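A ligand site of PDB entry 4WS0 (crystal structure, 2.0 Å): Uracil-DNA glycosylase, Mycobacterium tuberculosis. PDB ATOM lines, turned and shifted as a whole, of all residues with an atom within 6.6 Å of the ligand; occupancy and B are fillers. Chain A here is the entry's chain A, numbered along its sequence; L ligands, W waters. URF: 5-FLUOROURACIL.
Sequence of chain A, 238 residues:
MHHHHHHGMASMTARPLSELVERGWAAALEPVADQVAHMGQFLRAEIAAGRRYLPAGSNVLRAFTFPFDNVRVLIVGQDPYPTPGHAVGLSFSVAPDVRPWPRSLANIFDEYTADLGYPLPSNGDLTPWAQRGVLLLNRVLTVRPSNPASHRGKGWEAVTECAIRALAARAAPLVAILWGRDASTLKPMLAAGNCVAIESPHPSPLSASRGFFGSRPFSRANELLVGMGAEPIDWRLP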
ATOM      1  N   VAL A  76      -1.715 -19.795 -10.882  1.00  0.00           N
ATOM      2  CA  VAL A  76      -2.750 -18.890 -11.397  1.00  0.00           C
ATOM      3  C   VAL A  76      -2.565 -17.508 -10.812  1.00  0.00           C
ATOM      4  O   VAL A  76      -2.736 -17.311  -9.604  1.00  0.00           O
ATOM      5  CB  VAL A  76      -4.191 -19.325 -11.088  1.00  0.00           C
ATOM      6  CG1 VAL A  76      -5.197 -18.418 -11.815  1.00  0.00           C
ATOM      7  CG2 VAL A  76      -4.452 -20.784 -11.434  1.00  0.00           C
ATOM      8  N   GLY A  77      -2.250 -16.528 -11.659  1.00  0.00           N
ATOM      9  CA  GLY A  77      -2.278 -15.147 -11.248  1.00  0.00           C
ATOM     10  C   GLY A  77      -3.554 -14.447 -11.727  1.00  0.00           C
ATOM     11  O   GLY A  77      -4.551 -15.092 -12.077  1.00  0.00           O
ATOM     12  N   GLN A  78      -3.529 -13.119 -11.741  1.00  0.00           N
ATOM     13  CA  GLN A  78      -4.722 -12.303 -11.966  1.00  0.00           C
ATOM     14  C   GLN A  78      -4.840 -11.912 -13.433  1.00  0.00           C
ATOM     15  O   GLN A  78      -5.746 -12.345 -14.121  1.00  0.00           O
ATOM     16  CB  GLN A  78      -4.678 -11.091 -11.065  1.00  0.00           C
ATOM     17  CG  GLN A  78      -4.887 -11.479  -9.576  1.00  0.00           C
ATOM     18  CD  GLN A  78      -4.654 -10.370  -8.574  1.00  0.00           C
ATOM     19  OE1 GLN A  78      -4.641 -10.614  -7.371  1.00  0.00           O
ATOM     20  NE2 GLN A  78      -4.521  -9.121  -9.048  1.00  0.00           N
ATOM     21  N   ASP A  79      -3.907 -11.094 -13.917  1.00  0.00           N
ATOM     22  CA  ASP A  79      -4.009 -10.571 -15.270  1.00  0.00           C
ATOM     23  C   ASP A  79      -2.565 -10.305 -15.789  1.00  0.00           C
ATOM     24  O   ASP A  79      -1.622 -10.149 -14.997  1.00  0.00           O
ATOM     25  CB  ASP A  79      -4.758  -9.195 -15.247  1.00  0.00           C
ATOM     26  CG  ASP A  79      -6.116  -9.246 -14.576  1.00  0.00           C
ATOM     27  OD1 ASP A  79      -6.161  -9.242 -13.306  1.00  0.00           O
ATOM     28  OD2 ASP A  79      -7.133  -9.193 -15.321  1.00  0.00           O
ATOM     29  N   PRO A  80      -2.380 -10.191 -17.112  1.00  0.00           N
ATOM     30  CA  PRO A  80      -1.017 -10.033 -17.556  1.00  0.00           C
ATOM     31  C   PRO A  80      -0.333  -8.683 -17.217  1.00  0.00           C
ATOM     32  O   PRO A  80      -1.002  -7.687 -16.962  1.00  0.00           O
ATOM     33  CB  PRO A  80      -1.131 -10.237 -19.073  1.00  0.00           C
ATOM     34  CG  PRO A  80      -2.410 -10.952 -19.266  1.00  0.00           C
ATOM     35  CD  PRO A  80      -3.308 -10.364 -18.247  1.00  0.00           C
ATOM     36  N   TYR A  81       0.988  -8.669 -17.211  1.00  0.00           N
ATOM     37  CA  TYR A  81       1.757  -7.396 -17.123  1.00  0.00           C
ATOM     38  C   TYR A  81       1.181  -6.305 -18.052  1.00  0.00           C
ATOM     39  O   TYR A  81       0.961  -6.557 -19.240  1.00  0.00           O
ATOM     40  CB  TYR A  81       3.230  -7.622 -17.494  1.00  0.00           C
ATOM     41  CG  TYR A  81       4.015  -8.500 -16.559  1.00  0.00           C
ATOM     42  CD1 TYR A  81       4.140  -8.143 -15.207  1.00  0.00           C
ATOM     43  CD2 TYR A  81       4.721  -9.622 -17.021  1.00  0.00           C
ATOM     44  CE1 TYR A  81       4.874  -8.895 -14.339  1.00  0.00           C
ATOM     45  CE2 TYR A  81       5.464 -10.377 -16.176  1.00  0.00           C
ATOM     46  CZ  TYR A  81       5.555 -10.011 -14.813  1.00  0.00           C
ATOM     47  OH  TYR A  81       6.258 -10.697 -13.849  1.00  0.00           O
ATOM     48  N   PRO A  82       0.844  -5.126 -17.498  1.00  0.00           N
ATOM     49  CA  PRO A  82       0.283  -4.047 -18.356  1.00  0.00           C
ATOM     50  C   PRO A  82       1.288  -3.238 -19.171  1.00  0.00           C
ATOM     51  O   PRO A  82       0.874  -2.481 -20.062  1.00  0.00           O
ATOM     52  CB  PRO A  82      -0.483  -3.174 -17.380  1.00  0.00           C
ATOM     53  CG  PRO A  82       0.137  -3.409 -16.051  1.00  0.00           C
ATOM     54  CD  PRO A  82       0.786  -4.781 -16.062  1.00  0.00           C
ATOM     55  N   ALA A  87       4.646  -8.844 -20.793  1.00  0.00           N
ATOM     56  CA  ALA A  87       3.852 -10.046 -20.883  1.00  0.00           C
ATOM     57  C   ALA A  87       4.224 -10.894 -22.115  1.00  0.00           C
ATOM     58  O   ALA A  87       4.383 -10.376 -23.234  1.00  0.00           O
ATOM     59  CB  ALA A  87       2.369  -9.758 -20.902  1.00  0.00           C
ATOM     60  N   LEU A  90       2.955 -16.544 -20.758  1.00  0.00           N
ATOM     61  CA  LEU A  90       3.152 -17.385 -19.602  1.00  0.00           C
ATOM     62  C   LEU A  90       3.105 -16.447 -18.396  1.00  0.00           C
ATOM     63  O   LEU A  90       3.898 -15.519 -18.276  1.00  0.00           O
ATOM     64  CB  LEU A  90       4.477 -18.188 -19.688  1.00  0.00           C
ATOM     65  CG  LEU A  90       4.635 -19.108 -20.902  1.00  0.00           C
ATOM     66  CD1 LEU A  90       6.022 -19.699 -20.955  1.00  0.00           C
ATOM     67  CD2 LEU A  90       3.560 -20.228 -20.954  1.00  0.00           C
ATOM     68  N   SER A  91       2.152 -16.684 -17.491  1.00  0.00           N
ATOM     69  CA  SER A  91       2.003 -15.746 -16.347  1.00  0.00           C
ATOM     70  C   SER A  91       3.348 -15.516 -15.636  1.00  0.00           C
ATOM     71  O   SER A  91       4.143 -16.435 -15.380  1.00  0.00           O
ATOM     72  CB  SER A  91       0.905 -16.152 -15.347  1.00  0.00           C
ATOM     73  OG  SER A  91       1.216 -17.412 -14.763  1.00  0.00           O
ATOM     74  N   PHE A  92       3.579 -14.252 -15.347  1.00  0.00           N
ATOM     75  CA  PHE A  92       4.747 -13.742 -14.693  1.00  0.00           C
ATOM     76  C   PHE A  92       6.069 -13.742 -15.419  1.00  0.00           C
ATOM     77  O   PHE A  92       6.969 -12.992 -14.999  1.00  0.00           O
ATOM     78  CB  PHE A  92       4.896 -14.389 -13.306  1.00  0.00           C
ATOM     79  CG  PHE A  92       3.697 -14.207 -12.445  1.00  0.00           C
ATOM     80  CD1 PHE A  92       3.518 -13.032 -11.720  1.00  0.00           C
ATOM     81  CD2 PHE A  92       2.741 -15.200 -12.363  1.00  0.00           C
ATOM     82  CE1 PHE A  92       2.403 -12.860 -10.918  1.00  0.00           C
ATOM     83  CE2 PHE A  92       1.635 -15.024 -11.533  1.00  0.00           C
ATOM     84  CZ  PHE A  92       1.499 -13.869 -10.787  1.00  0.00           C
ATOM     85  N   SER A  93       6.169 -14.501 -16.521  1.00  0.00           N
ATOM     86  CA  SER A  93       7.388 -14.636 -17.214  1.00  0.00           C
ATOM     87  C   SER A  93       7.750 -13.389 -18.040  1.00  0.00           C
ATOM     88  O   SER A  93       6.889 -12.642 -18.536  1.00  0.00           O
ATOM     89  CB  SER A  93       7.328 -15.845 -18.142  1.00  0.00           C
ATOM     90  OG  SER A  93       8.582 -16.236 -18.628  1.00  0.00           O
ATOM     91  N   PRO A 102      10.116  -7.248 -13.961  1.00  0.00           N
ATOM     92  CA  PRO A 102       8.980  -6.638 -13.249  1.00  0.00           C
ATOM     93  C   PRO A 102       9.018  -6.996 -11.761  1.00  0.00           C
ATOM     94  O   PRO A 102       9.578  -8.044 -11.397  1.00  0.00           O
ATOM     95  CB  PRO A 102       7.757  -7.280 -13.886  1.00  0.00           C
ATOM     96  CG  PRO A 102       8.223  -7.674 -15.269  1.00  0.00           C
ATOM     97  CD  PRO A 102       9.657  -8.081 -15.100  1.00  0.00           C
ATOM     98  N   SER A 104       6.805  -8.061  -9.602  1.00  0.00           N
ATOM     99  CA  SER A 104       6.118  -9.330  -9.228  1.00  0.00           C
ATOM    100  C   SER A 104       7.100 -10.501  -9.423  1.00  0.00           C
ATOM    101  O   SER A 104       7.176 -11.420  -8.555  1.00  0.00           O
ATOM    102  CB  SER A 104       4.839  -9.584 -10.096  1.00  0.00           C
ATOM    103  OG  SER A 104       3.717  -8.819  -9.624  1.00  0.00           O
ATOM    104  N   LEU A 137      -0.788 -19.746 -15.645  1.00  0.00           N
ATOM    105  CA  LEU A 137      -2.044 -19.287 -16.105  1.00  0.00           C
ATOM    106  C   LEU A 137      -2.340 -17.957 -15.407  1.00  0.00           C
ATOM    107  O   LEU A 137      -1.799 -17.683 -14.361  1.00  0.00           O
ATOM    108  CB  LEU A 137      -3.088 -20.386 -15.744  1.00  0.00           C
ATOM    109  CG  LEU A 137      -4.542 -20.161 -16.168  1.00  0.00           C
ATOM    110  CD1 LEU A 137      -4.583 -20.044 -17.683  1.00  0.00           C
ATOM    111  CD2 LEU A 137      -5.512 -21.262 -15.714  1.00  0.00           C
ATOM    112  N   ASN A 138      -3.181 -17.152 -15.992  1.00  0.00           N
ATOM    113  CA  ASN A 138      -3.809 -16.041 -15.353  1.00  0.00           C
ATOM    114  C   ASN A 138      -5.320 -16.240 -15.428  1.00  0.00           C
ATOM    115  O   ASN A 138      -5.849 -16.817 -16.348  1.00  0.00           O
ATOM    116  CB  ASN A 138      -3.459 -14.726 -16.069  1.00  0.00           C
ATOM    117  CG  ASN A 138      -2.124 -14.166 -15.669  1.00  0.00           C
ATOM    118  OD1 ASN A 138      -1.865 -14.011 -14.502  1.00  0.00           O
ATOM    119  ND2 ASN A 138      -1.280 -13.859 -16.602  1.00  0.00           N
ATOM    120  N   TRP A 179      -2.384 -17.268  -6.461  1.00  0.00           N
ATOM    121  CA  TRP A 179      -1.761 -16.004  -5.993  1.00  0.00           C
ATOM    122  C   TRP A 179      -2.702 -14.850  -6.267  1.00  0.00           C
ATOM    123  O   TRP A 179      -2.864 -14.385  -7.400  1.00  0.00           O
ATOM    124  CB  TRP A 179      -0.430 -15.719  -6.680  1.00  0.00           C
ATOM    125  CG  TRP A 179       0.742 -16.632  -6.294  1.00  0.00           C
ATOM    126  CD1 TRP A 179       0.910 -17.284  -5.125  1.00  0.00           C
ATOM    127  CD2 TRP A 179       1.905 -16.925  -7.084  1.00  0.00           C
ATOM    128  NE1 TRP A 179       2.095 -17.945  -5.101  1.00  0.00           N
ATOM    129  CE2 TRP A 179       2.714 -17.785  -6.309  1.00  0.00           C
ATOM    130  CE3 TRP A 179       2.353 -16.554  -8.383  1.00  0.00           C
ATOM    131  CZ2 TRP A 179       3.973 -18.257  -6.763  1.00  0.00           C
ATOM    132  CZ3 TRP A 179       3.577 -17.068  -8.841  1.00  0.00           C
ATOM    133  CH2 TRP A 179       4.362 -17.929  -8.026  1.00  0.00           C
ATOM    134  N   HIS A 202      -0.864 -11.981  -3.516  1.00  0.00           N
ATOM    135  CA  HIS A 202      -0.181 -11.875  -4.791  1.00  0.00           C
ATOM    136  C   HIS A 202       1.237 -11.291  -4.603  1.00  0.00           C
ATOM    137  O   HIS A 202       1.468 -10.460  -3.643  1.00  0.00           O
ATOM    138  CB  HIS A 202      -1.103 -11.017  -5.687  1.00  0.00           C
ATOM    139  CG  HIS A 202      -0.716 -10.947  -7.134  1.00  0.00           C
ATOM    140  ND1 HIS A 202       0.323 -10.148  -7.588  1.00  0.00           N
ATOM    141  CD2 HIS A 202      -1.266 -11.502  -8.242  1.00  0.00           C
ATOM    142  CE1 HIS A 202       0.418 -10.251  -8.891  1.00  0.00           C
ATOM    143  NE2 HIS A 202      -0.542 -11.038  -9.328  1.00  0.00           N
ATOM    144  N   PRO A 203       2.213 -11.685  -5.464  1.00  0.00           N
ATOM    145  CA  PRO A 203       3.589 -11.113  -5.357  1.00  0.00           C
ATOM    146  C   PRO A 203       3.855  -9.683  -5.892  1.00  0.00           C
ATOM    147  O   PRO A 203       5.047  -9.201  -5.923  1.00  0.00           O
ATOM    148  CB  PRO A 203       4.410 -12.079  -6.188  1.00  0.00           C
ATOM    149  CG  PRO A 203       3.451 -12.530  -7.271  1.00  0.00           C
ATOM    150  CD  PRO A 203       2.172 -12.722  -6.531  1.00  0.00           C
ATOM    151  N   SER A 204       2.808  -8.957  -6.269  1.00  0.00           N
ATOM    152  CA  SER A 204       2.985  -7.592  -6.723  1.00  0.00           C
ATOM    153  C   SER A 204       3.442  -6.642  -5.569  1.00  0.00           C
ATOM    154  O   SER A 204       3.228  -6.967  -4.364  1.00  0.00           O
ATOM    155  CB  SER A 204       1.686  -7.069  -7.327  1.00  0.00           C
ATOM    156  OG  SER A 204       0.759  -6.719  -6.327  1.00  0.00           O
HETATM  157  N1  URF L   1       0.527 -10.246 -12.322  1.00  0.00           N
HETATM  158  C2  URF L   1      -0.301 -11.279 -12.575  1.00  0.00           C
HETATM  159  N3  URF L   1      -0.130 -12.107 -13.605  1.00  0.00           N
HETATM  160  C4  URF L   1       0.867 -11.958 -14.469  1.00  0.00           C
HETATM  161  C5  URF L   1       1.765 -10.869 -14.173  1.00  0.00           C
HETATM  162  C6  URF L   1       1.564 -10.044 -13.122  1.00  0.00           C
HETATM  163  O2  URF L   1      -1.254 -11.513 -11.788  1.00  0.00           O
HETATM  164  O4  URF L   1       1.126 -12.698 -15.477  1.00  0.00           O
HETATM  165  F5  URF L   1       2.775 -10.752 -15.015  1.00  0.00           F
HETATM  166  O   HOH W   1       2.133 -11.601 -18.081  1.00  0.00           O
HETATM  167  O   HOH W   2      -1.358  -7.792 -13.328  1.00  0.00           O
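An oxygen (O2) of the ligand sits at hydrogen-bond distance from a ring nitrogen (NE2) of His 202 (2.6 Å).
A nitrogen (N3) of the ligand sits at hydrogen-bond distance from the side-chain amide oxygen (OD1) of Asn 138.
N of Gln 78 lies within hydrogen-bond range of O2 of the ligand (2.8 Å).
The backbone NH (N) of Asp 79 sits at hydrogen-bond distance from an oxygen (O2) of the ligand (3.4 Å).
A nitrogen (N3) of the ligand lies within hydrogen-bond range of the backbone carbonyl oxygen (O) of Asp 79 (2.8 Å).
The backbone NH (N) of Phe 92 sits at hydrogen-bond distance from an oxygen (O4) of the ligand.
A ring nitrogen (ND1) of His 202 is in hydrogen-bond range of the backbone NH (N) of Ser 204.
N of Gln 78 lies within hydrogen-bond range of OD1 of Asn 138 (3.3 Å).
O of Phe 92 is in hydrogen-bond range of OH of Tyr 81.
O of Leu 137 lies within hydrogen-bond range of OG of Ser 91 (3.1 Å).
The backbone carbonyl oxygen of Leu 137 lies within hydrogen-bond range of the backbone NH of Gly 77, at 3.0 Å.
Gly 77 touches the ligand.
Tyr 81 touches the ligand.
CA of Ser 91 touches O4 of the ligand, 3.3 Å away.
Along chain A the residues within 4 Å of the ligand span positions 77 to 202.
The nearest printed residue that does not touch the ligand is Pro 80 (4.002 Å).
Water W1 bridges an oxygen (O4) of the ligand (3.0 Å) and the backbone NH of Tyr 81 (3.3 Å).
Water W2 bridges O of Asp 79 (2.9 Å) and N1 of the ligand (3.3 Å).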
